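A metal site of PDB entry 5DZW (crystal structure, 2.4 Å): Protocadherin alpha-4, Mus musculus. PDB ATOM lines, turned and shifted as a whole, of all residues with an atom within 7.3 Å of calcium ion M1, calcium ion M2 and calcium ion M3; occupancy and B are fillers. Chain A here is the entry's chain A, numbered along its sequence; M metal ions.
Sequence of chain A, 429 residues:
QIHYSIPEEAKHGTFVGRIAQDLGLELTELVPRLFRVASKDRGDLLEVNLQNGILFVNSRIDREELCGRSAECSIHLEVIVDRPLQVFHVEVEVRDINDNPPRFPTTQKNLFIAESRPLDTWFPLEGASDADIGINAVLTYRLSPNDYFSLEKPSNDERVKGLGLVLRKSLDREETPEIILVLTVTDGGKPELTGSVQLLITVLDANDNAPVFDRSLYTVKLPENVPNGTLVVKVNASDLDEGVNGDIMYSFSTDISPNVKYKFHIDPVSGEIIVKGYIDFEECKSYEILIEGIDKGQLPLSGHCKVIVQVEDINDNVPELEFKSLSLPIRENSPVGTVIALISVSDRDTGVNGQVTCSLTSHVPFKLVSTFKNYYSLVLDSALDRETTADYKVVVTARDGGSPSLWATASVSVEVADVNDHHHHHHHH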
ATOM      1  N   GLU A 115      11.560 -29.720 -17.165  1.00  0.00           N
ATOM      2  CA  GLU A 115      11.608 -28.261 -17.054  1.00  0.00           C
ATOM      3  C   GLU A 115      11.093 -27.803 -15.686  1.00  0.00           C
ATOM      4  O   GLU A 115      11.393 -26.695 -15.242  1.00  0.00           O
ATOM      5  CB  GLU A 115      10.774 -27.632 -18.169  1.00  0.00           C
ATOM      6  CG  GLU A 115      10.849 -26.117 -18.251  1.00  0.00           C
ATOM      7  CD  GLU A 115       9.823 -25.531 -19.192  1.00  0.00           C
ATOM      8  OE1 GLU A 115       9.085 -26.307 -19.836  1.00  0.00           O
ATOM      9  OE2 GLU A 115       9.740 -24.286 -19.285  1.00  0.00           O
ATOM     10  N   LEU A 171      15.433 -23.325 -15.864  1.00  0.00           N
ATOM     11  CA  LEU A 171      15.479 -23.900 -17.207  1.00  0.00           C
ATOM     12  C   LEU A 171      14.139 -23.746 -17.922  1.00  0.00           C
ATOM     13  O   LEU A 171      13.078 -23.923 -17.322  1.00  0.00           O
ATOM     14  CB  LEU A 171      15.882 -25.376 -17.139  1.00  0.00           C
ATOM     15  CG  LEU A 171      14.899 -26.432 -16.625  1.00  0.00           C
ATOM     16  CD1 LEU A 171      15.423 -27.825 -16.925  1.00  0.00           C
ATOM     17  CD2 LEU A 171      14.625 -26.287 -15.125  1.00  0.00           C
ATOM     18  N   ASP A 172      14.195 -23.419 -19.205  1.00  0.00           N
ATOM     19  CA  ASP A 172      12.999 -23.221 -20.005  1.00  0.00           C
ATOM     20  C   ASP A 172      13.097 -23.954 -21.346  1.00  0.00           C
ATOM     21  O   ASP A 172      13.968 -23.656 -22.155  1.00  0.00           O
ATOM     22  CB  ASP A 172      12.746 -21.727 -20.235  1.00  0.00           C
ATOM     23  CG  ASP A 172      11.488 -21.464 -21.049  1.00  0.00           C
ATOM     24  OD1 ASP A 172      10.392 -21.446 -20.442  1.00  0.00           O
ATOM     25  OD2 ASP A 172      11.592 -21.275 -22.275  1.00  0.00           O
ATOM     26  N   ARG A 173      12.186 -24.890 -21.561  1.00  0.00           N
ATOM     27  CA  ARG A 173      12.165 -25.709 -22.763  1.00  0.00           C
ATOM     28  C   ARG A 173      11.995 -24.870 -24.040  1.00  0.00           C
ATOM     29  O   ARG A 173      12.630 -25.153 -25.056  1.00  0.00           O
ATOM     30  CB  ARG A 173      11.067 -26.761 -22.663  1.00  0.00           C
ATOM     31  CG  ARG A 173      10.721 -27.467 -23.959  1.00  0.00           C
ATOM     32  CD  ARG A 173       9.359 -27.020 -24.478  1.00  0.00           C
ATOM     33  NE  ARG A 173       8.888 -27.855 -25.576  1.00  0.00           N
ATOM     34  CZ  ARG A 173       9.122 -27.596 -26.861  1.00  0.00           C
ATOM     35  NH1 ARG A 173       8.655 -28.405 -27.802  1.00  0.00           N
ATOM     36  NH2 ARG A 173       9.824 -26.528 -27.204  1.00  0.00           N
ATOM     37  N   GLU A 174      11.144 -23.859 -23.975  1.00  0.00           N
ATOM     38  CA  GLU A 174      10.849 -23.028 -25.133  1.00  0.00           C
ATOM     39  C   GLU A 174      12.039 -22.174 -25.566  1.00  0.00           C
ATOM     40  O   GLU A 174      12.263 -21.960 -26.749  1.00  0.00           O
ATOM     41  CB  GLU A 174       9.635 -22.127 -24.866  1.00  0.00           C
ATOM     42  CG  GLU A 174       8.297 -22.845 -24.886  1.00  0.00           C
ATOM     43  CD  GLU A 174       8.087 -23.747 -23.685  1.00  0.00           C
ATOM     44  OE1 GLU A 174       8.772 -23.543 -22.661  1.00  0.00           O
ATOM     45  OE2 GLU A 174       7.240 -24.665 -23.771  1.00  0.00           O
ATOM     46  N   GLU A 175      12.796 -21.693 -24.582  1.00  0.00           N
ATOM     47  CA  GLU A 175      13.970 -20.871 -24.871  1.00  0.00           C
ATOM     48  C   GLU A 175      15.102 -21.710 -25.467  1.00  0.00           C
ATOM     49  O   GLU A 175      15.613 -21.400 -26.547  1.00  0.00           O
ATOM     50  CB  GLU A 175      14.452 -20.166 -23.600  1.00  0.00           C
ATOM     51  CG  GLU A 175      15.673 -19.285 -23.799  1.00  0.00           C
ATOM     52  CD  GLU A 175      16.031 -18.484 -22.567  1.00  0.00           C
ATOM     53  OE1 GLU A 175      15.120 -18.232 -21.742  1.00  0.00           O
ATOM     54  OE2 GLU A 175      17.205 -18.104 -22.411  1.00  0.00           O
ATOM     55  N   LEU A 204      12.512 -31.506 -20.965  1.00  0.00           N
ATOM     56  CA  LEU A 204      11.156 -31.951 -21.240  1.00  0.00           C
ATOM     57  C   LEU A 204      10.160 -30.799 -21.123  1.00  0.00           C
ATOM     58  O   LEU A 204      10.371 -29.854 -20.365  1.00  0.00           O
ATOM     59  CB  LEU A 204      10.772 -33.092 -20.297  1.00  0.00           C
ATOM     60  CG  LEU A 204      11.762 -34.256 -20.242  1.00  0.00           C
ATOM     61  CD1 LEU A 204      11.329 -35.318 -19.239  1.00  0.00           C
ATOM     62  CD2 LEU A 204      11.963 -34.865 -21.628  1.00  0.00           C
ATOM     63  N   ASP A 205       9.074 -30.882 -21.890  1.00  0.00           N
ATOM     64  CA  ASP A 205       8.081 -29.805 -21.919  1.00  0.00           C
ATOM     65  C   ASP A 205       7.162 -29.837 -20.698  1.00  0.00           C
ATOM     66  O   ASP A 205       6.439 -30.813 -20.480  1.00  0.00           O
ATOM     67  CB  ASP A 205       7.252 -29.889 -23.198  1.00  0.00           C
ATOM     68  CG  ASP A 205       6.218 -28.779 -23.298  1.00  0.00           C
ATOM     69  OD1 ASP A 205       6.514 -27.650 -22.865  1.00  0.00           O
ATOM     70  OD2 ASP A 205       5.111 -29.040 -23.812  1.00  0.00           O
ATOM     71  N   ALA A 206       7.202 -28.775 -19.912  1.00  0.00           N
ATOM     72  CA  ALA A 206       6.309 -28.626 -18.767  1.00  0.00           C
ATOM     73  C   ALA A 206       5.137 -27.723 -19.140  1.00  0.00           C
ATOM     74  O   ALA A 206       5.246 -26.915 -20.051  1.00  0.00           O
ATOM     75  CB  ALA A 206       7.058 -28.079 -17.573  1.00  0.00           C
ATOM     76  N   ASN A 207       4.036 -27.864 -18.424  1.00  0.00           N
ATOM     77  CA  ASN A 207       2.857 -27.027 -18.683  1.00  0.00           C
ATOM     78  C   ASN A 207       2.899 -25.753 -17.839  1.00  0.00           C
ATOM     79  O   ASN A 207       2.107 -25.576 -16.921  1.00  0.00           O
ATOM     80  CB  ASN A 207       1.572 -27.803 -18.398  1.00  0.00           C
ATOM     81  CG  ASN A 207       0.342 -27.088 -18.917  1.00  0.00           C
ATOM     82  OD1 ASN A 207       0.413 -26.303 -19.858  1.00  0.00           O
ATOM     83  ND2 ASN A 207      -0.804 -27.344 -18.284  1.00  0.00           N
ATOM     84  N   ASP A 208       3.842 -24.875 -18.163  1.00  0.00           N
ATOM     85  CA  ASP A 208       4.056 -23.668 -17.377  1.00  0.00           C
ATOM     86  C   ASP A 208       3.786 -22.393 -18.178  1.00  0.00           C
ATOM     87  O   ASP A 208       4.143 -21.294 -17.752  1.00  0.00           O
ATOM     88  CB  ASP A 208       5.484 -23.640 -16.821  1.00  0.00           C
ATOM     89  CG  ASP A 208       6.535 -23.775 -17.905  1.00  0.00           C
ATOM     90  OD1 ASP A 208       6.278 -24.485 -18.899  1.00  0.00           O
ATOM     91  OD2 ASP A 208       7.620 -23.169 -17.753  1.00  0.00           O
ATOM     92  N   ASN A 209       3.151 -22.539 -19.340  1.00  0.00           N
ATOM     93  CA  ASN A 209       2.780 -21.395 -20.150  1.00  0.00           C
ATOM     94  C   ASN A 209       1.297 -21.382 -20.508  1.00  0.00           C
ATOM     95  O   ASN A 209       0.771 -22.361 -21.047  1.00  0.00           O
ATOM     96  CB  ASN A 209       3.615 -21.341 -21.430  1.00  0.00           C
ATOM     97  CG  ASN A 209       4.973 -20.688 -21.218  1.00  0.00           C
ATOM     98  OD1 ASN A 209       5.564 -20.815 -20.147  1.00  0.00           O
ATOM     99  ND2 ASN A 209       5.451 -19.984 -22.233  1.00  0.00           N
ATOM    100  N   ALA A 210       0.628 -20.280 -20.192  1.00  0.00           N
ATOM    101  CA  ALA A 210      -0.796 -20.127 -20.483  1.00  0.00           C
ATOM    102  C   ALA A 210      -1.003 -19.645 -21.919  1.00  0.00           C
ATOM    103  O   ALA A 210      -0.158 -18.943 -22.473  1.00  0.00           O
ATOM    104  CB  ALA A 210      -1.424 -19.154 -19.497  1.00  0.00           C
ATOM    105  N   PRO A 211      -2.141 -20.028 -22.531  1.00  0.00           N
ATOM    106  CA  PRO A 211      -2.475 -19.566 -23.872  1.00  0.00           C
ATOM    107  C   PRO A 211      -2.680 -18.057 -23.937  1.00  0.00           C
ATOM    108  O   PRO A 211      -3.085 -17.454 -22.940  1.00  0.00           O
ATOM    109  CB  PRO A 211      -3.779 -20.311 -24.186  1.00  0.00           C
ATOM    110  CG  PRO A 211      -4.329 -20.715 -22.865  1.00  0.00           C
ATOM    111  CD  PRO A 211      -3.132 -20.978 -22.003  1.00  0.00           C
ATOM    112  N   ASP A 239      -0.184 -20.836 -27.840  1.00  0.00           N
ATOM    113  CA  ASP A 239       0.454 -21.330 -26.628  1.00  0.00           C
ATOM    114  C   ASP A 239       1.808 -21.961 -26.947  1.00  0.00           C
ATOM    115  O   ASP A 239       1.939 -22.712 -27.912  1.00  0.00           O
ATOM    116  CB  ASP A 239      -0.461 -22.333 -25.915  1.00  0.00           C
ATOM    117  CG  ASP A 239       0.044 -22.715 -24.536  1.00  0.00           C
ATOM    118  OD1 ASP A 239       0.944 -22.013 -24.012  1.00  0.00           O
ATOM    119  OD2 ASP A 239      -0.458 -23.704 -23.978  1.00  0.00           O
ATOM    120  N   LEU A 240       2.806 -21.653 -26.117  1.00  0.00           N
ATOM    121  CA  LEU A 240       4.179 -22.048 -26.403  1.00  0.00           C
ATOM    122  C   LEU A 240       4.467 -23.518 -26.100  1.00  0.00           C
ATOM    123  O   LEU A 240       5.399 -24.093 -26.650  1.00  0.00           O
ATOM    124  CB  LEU A 240       5.146 -21.160 -25.617  1.00  0.00           C
ATOM    125  CG  LEU A 240       5.183 -19.699 -26.048  1.00  0.00           C
ATOM    126  CD1 LEU A 240       6.231 -18.923 -25.266  1.00  0.00           C
ATOM    127  CD2 LEU A 240       5.450 -19.589 -27.547  1.00  0.00           C
ATOM    128  N   ASP A 241       3.660 -24.123 -25.238  1.00  0.00           N
ATOM    129  CA  ASP A 241       3.848 -25.532 -24.899  1.00  0.00           C
ATOM    130  C   ASP A 241       3.411 -26.441 -26.041  1.00  0.00           C
ATOM    131  O   ASP A 241       2.727 -26.000 -26.970  1.00  0.00           O
ATOM    132  CB  ASP A 241       3.091 -25.884 -23.614  1.00  0.00           C
ATOM    133  CG  ASP A 241       3.554 -25.080 -22.423  1.00  0.00           C
ATOM    134  OD1 ASP A 241       4.525 -24.309 -22.565  1.00  0.00           O
ATOM    135  OD2 ASP A 241       2.963 -25.228 -21.336  1.00  0.00           O
ATOM    136  N   GLU A 242       3.810 -27.705 -25.973  1.00  0.00           N
ATOM    137  CA  GLU A 242       3.516 -28.658 -27.042  1.00  0.00           C
ATOM    138  C   GLU A 242       2.638 -29.810 -26.553  1.00  0.00           C
ATOM    139  O   GLU A 242       2.451 -29.992 -25.352  1.00  0.00           O
ATOM    140  CB  GLU A 242       4.815 -29.204 -27.634  1.00  0.00           C
ATOM    141  N   VAL A 244      -0.649 -31.954 -25.681  1.00  0.00           N
ATOM    142  CA  VAL A 244      -1.923 -31.598 -25.090  1.00  0.00           C
ATOM    143  C   VAL A 244      -1.790 -30.321 -24.259  1.00  0.00           C
ATOM    144  O   VAL A 244      -2.777 -29.662 -23.949  1.00  0.00           O
ATOM    145  CB  VAL A 244      -2.485 -32.726 -24.204  1.00  0.00           C
ATOM    146  CG1 VAL A 244      -2.800 -33.957 -25.036  1.00  0.00           C
ATOM    147  CG2 VAL A 244      -1.507 -33.072 -23.083  1.00  0.00           C
ATOM    148  N   ASN A 245      -0.549 -29.981 -23.900  1.00  0.00           N
ATOM    149  CA  ASN A 245      -0.278 -28.753 -23.175  1.00  0.00           C
ATOM    150  C   ASN A 245      -0.305 -27.545 -24.102  1.00  0.00           C
ATOM    151  O   ASN A 245      -0.261 -26.405 -23.649  1.00  0.00           O
ATOM    152  CB  ASN A 245       1.073 -28.835 -22.463  1.00  0.00           C
ATOM    153  CG  ASN A 245       1.118 -29.944 -21.424  1.00  0.00           C
ATOM    154  OD1 ASN A 245       0.170 -30.706 -21.282  1.00  0.00           O
ATOM    155  ND2 ASN A 245       2.227 -30.028 -20.711  1.00  0.00           N
ATOM    156  N   GLY A 246      -0.393 -27.814 -25.399  1.00  0.00           N
ATOM    157  CA  GLY A 246      -0.420 -26.761 -26.400  1.00  0.00           C
ATOM    158  C   GLY A 246      -1.790 -26.555 -27.025  1.00  0.00           C
ATOM    159  O   GLY A 246      -2.143 -25.444 -27.423  1.00  0.00           O
ATOM    160  N   ASP A 247      -2.569 -27.637 -27.124  1.00  0.00           N
ATOM    161  CA  ASP A 247      -3.907 -27.563 -27.710  1.00  0.00           C
ATOM    162  C   ASP A 247      -4.852 -26.753 -26.833  1.00  0.00           C
ATOM    163  O   ASP A 247      -4.890 -26.935 -25.620  1.00  0.00           O
ATOM    164  CB  ASP A 247      -4.466 -28.970 -27.938  1.00  0.00           C
ATOM    165  CG  ASP A 247      -3.788 -29.693 -29.084  1.00  0.00           C
ATOM    166  OD1 ASP A 247      -2.570 -29.494 -29.281  1.00  0.00           O
ATOM    167  OD2 ASP A 247      -4.468 -30.463 -29.788  1.00  0.00           O
ATOM    168  N   ILE A 248      -5.619 -25.856 -27.463  1.00  0.00           N
ATOM    169  CA  ILE A 248      -6.479 -24.937 -26.728  1.00  0.00           C
ATOM    170  C   ILE A 248      -7.962 -25.145 -27.024  1.00  0.00           C
ATOM    171  O   ILE A 248      -8.372 -25.227 -28.179  1.00  0.00           O
ATOM    172  CB  ILE A 248      -6.115 -23.475 -27.056  1.00  0.00           C
ATOM    173  CG1 ILE A 248      -4.603 -23.253 -26.945  1.00  0.00           C
ATOM    174  CG2 ILE A 248      -6.867 -22.512 -26.138  1.00  0.00           C
ATOM    175  CD1 ILE A 248      -4.150 -21.893 -27.415  1.00  0.00           C
ATOM    176  N   ASP A 295      -5.941 -24.750 -22.038  1.00  0.00           N
ATOM    177  CA  ASP A 295      -5.199 -25.862 -22.630  1.00  0.00           C
ATOM    178  C   ASP A 295      -5.654 -27.195 -22.059  1.00  0.00           C
ATOM    179  O   ASP A 295      -6.526 -27.252 -21.192  1.00  0.00           O
ATOM    180  CB  ASP A 295      -3.685 -25.677 -22.431  1.00  0.00           C
ATOM    181  CG  ASP A 295      -3.326 -25.249 -21.025  1.00  0.00           C
ATOM    182  OD1 ASP A 295      -4.002 -25.687 -20.071  1.00  0.00           O
ATOM    183  OD2 ASP A 295      -2.361 -24.477 -20.862  1.00  0.00           O
ATOM    184  N   LYS A 296      -5.065 -28.288 -22.543  1.00  0.00           N
ATOM    185  CA  LYS A 296      -5.495 -29.629 -22.160  1.00  0.00           C
ATOM    186  C   LYS A 296      -4.416 -30.392 -21.403  1.00  0.00           C
ATOM    187  O   LYS A 296      -4.213 -31.583 -21.638  1.00  0.00           O
ATOM    188  CB  LYS A 296      -5.918 -30.414 -23.409  1.00  0.00           C
ATOM    189  CG  LYS A 296      -6.981 -29.734 -24.251  1.00  0.00           C
ATOM    190  CD  LYS A 296      -7.301 -30.545 -25.499  1.00  0.00           C
ATOM    191  N   GLY A 297      -3.729 -29.710 -20.492  1.00  0.00           N
ATOM    192  CA  GLY A 297      -2.697 -30.336 -19.694  1.00  0.00           C
ATOM    193  C   GLY A 297      -3.249 -30.931 -18.419  1.00  0.00           C
ATOM    194  O   GLY A 297      -4.446 -30.824 -18.138  1.00  0.00           O
ATOM    195  N   LEU A 299      -2.448 -29.980 -15.310  1.00  0.00           N
ATOM    196  CA  LEU A 299      -2.852 -28.774 -14.604  1.00  0.00           C
ATOM    197  C   LEU A 299      -3.116 -27.680 -15.622  1.00  0.00           C
ATOM    198  O   LEU A 299      -2.181 -26.999 -16.060  1.00  0.00           O
ATOM    199  CB  LEU A 299      -1.791 -28.335 -13.595  1.00  0.00           C
ATOM    200  CG  LEU A 299      -2.130 -27.090 -12.781  1.00  0.00           C
ATOM    201  CD1 LEU A 299      -3.466 -27.260 -12.074  1.00  0.00           C
ATOM    202  CD2 LEU A 299      -1.026 -26.767 -11.793  1.00  0.00           C
ATOM    203  N   PRO A 300      -4.385 -27.510 -16.017  1.00  0.00           N
ATOM    204  CA  PRO A 300      -4.784 -26.584 -17.084  1.00  0.00           C
ATOM    205  C   PRO A 300      -4.467 -25.131 -16.775  1.00  0.00           C
ATOM    206  O   PRO A 300      -4.659 -24.680 -15.637  1.00  0.00           O
ATOM    207  CB  PRO A 300      -6.294 -26.799 -17.183  1.00  0.00           C
ATOM    208  CG  PRO A 300      -6.545 -28.141 -16.577  1.00  0.00           C
ATOM    209  CD  PRO A 300      -5.536 -28.263 -15.483  1.00  0.00           C
ATOM    210  N   LEU A 301      -3.989 -24.406 -17.779  1.00  0.00           N
ATOM    211  CA  LEU A 301      -3.799 -22.962 -17.670  1.00  0.00           C
ATOM    212  C   LEU A 301      -4.782 -22.244 -18.595  1.00  0.00           C
ATOM    213  O   LEU A 301      -5.092 -22.730 -19.687  1.00  0.00           O
ATOM    214  CB  LEU A 301      -2.363 -22.576 -18.022  1.00  0.00           C
ATOM    215  CG  LEU A 301      -1.288 -23.023 -17.028  1.00  0.00           C
ATOM    216  CD1 LEU A 301       0.070 -22.459 -17.415  1.00  0.00           C
ATOM    217  CD2 LEU A 301      -1.664 -22.609 -15.612  1.00  0.00           C
HETATM  218 CA    CA M   1       7.886 -23.179 -20.424  1.00  0.00          CA
HETATM  219 CA    CA M   2       6.564 -25.589 -21.507  1.00  0.00          CA
HETATM  220 CA    CA M   3       0.211 -24.588 -21.886  1.00  0.00          CA
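OD2 of Asp 172 is in hydrogen-bond range of N of Glu 174 (3.1 Å). The side-chain carboxylate (OD1) of Asp 295 sits at hydrogen-bond distance from the backbone NH (N) of Leu 301 (2.6 Å). O of Leu 204 sits close to N of Glu 115, at 3.4 Å. The side-chain carboxylate (OD1) of Asp 205 sits close to the guanidinium group (NE) of Arg 173 (3.6 Å). ND2 of Asn 207 sits at hydrogen-bond distance from O of Leu 299 (2.6 Å). OD2 of Asp 205 lies within hydrogen-bond range of N of Glu 242 (2.9 Å). The side-chain carboxylate of Glu 115 lies close to the backbone NH of Arg 173 (3.4 Å). OE1 of Glu 115 is in hydrogen-bond range of N of Ala 206 (3.1 Å).
Within 4 Å of calcium ion M1: Glu 115, Asp 172, Glu 174, Asp 208 and Asn 209. Along chain A the residues within 4 Å of calcium ion M1 span positions 115 to 209.
Of the 29 residues printed, 6 come within 4 Å of calcium ion M2. The nearest printed residue that does not touch calcium ion M2 is Arg 173 (4.3 Å).
Calcium ion M1 is bound by OE1 of Glu 174 (2.4 Å). OE2 of Glu 115 binds calcium ion M1 (2.4 Å). OD1 of Asp 208 binds calcium ion M1, 2.6 Å away. The side-chain carboxylate (OD2) of Asp 208 is bound to calcium ion M1 (2.7 Å). Slightly farther from calcium ion M1 lies OD1 of Asp 172 (3.0 Å).
Calcium ion M2 is bound by the backbone carbonyl oxygen (O) of Ala 206 (2.4 Å), the side-chain carboxylate (OD1) of Asp 205 (2.5 Å), the side-chain carboxylate (OE2) of Glu 174 (2.5 Å), the side-chain carboxylate (OD1) of Asp 241 (2.6 Å) and the side-chain carboxylate (OD1) of Asp 208 (2.8 Å). Calcium ion M2 has five donor atoms within binding distance. Slightly farther from calcium ion M2 lies OE1 of Glu 115 (3.1 Å).
Calcium ion M3 is bound by the side-chain carboxylate of Asp 239, the backbone carbonyl oxygen of Asn 209, the backbone carbonyl oxygen of Asn 245, the side-chain amide oxygen of Asn 207, the side-chain carboxylate of Asp 295 and the side-chain carboxylate of Asp 241.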
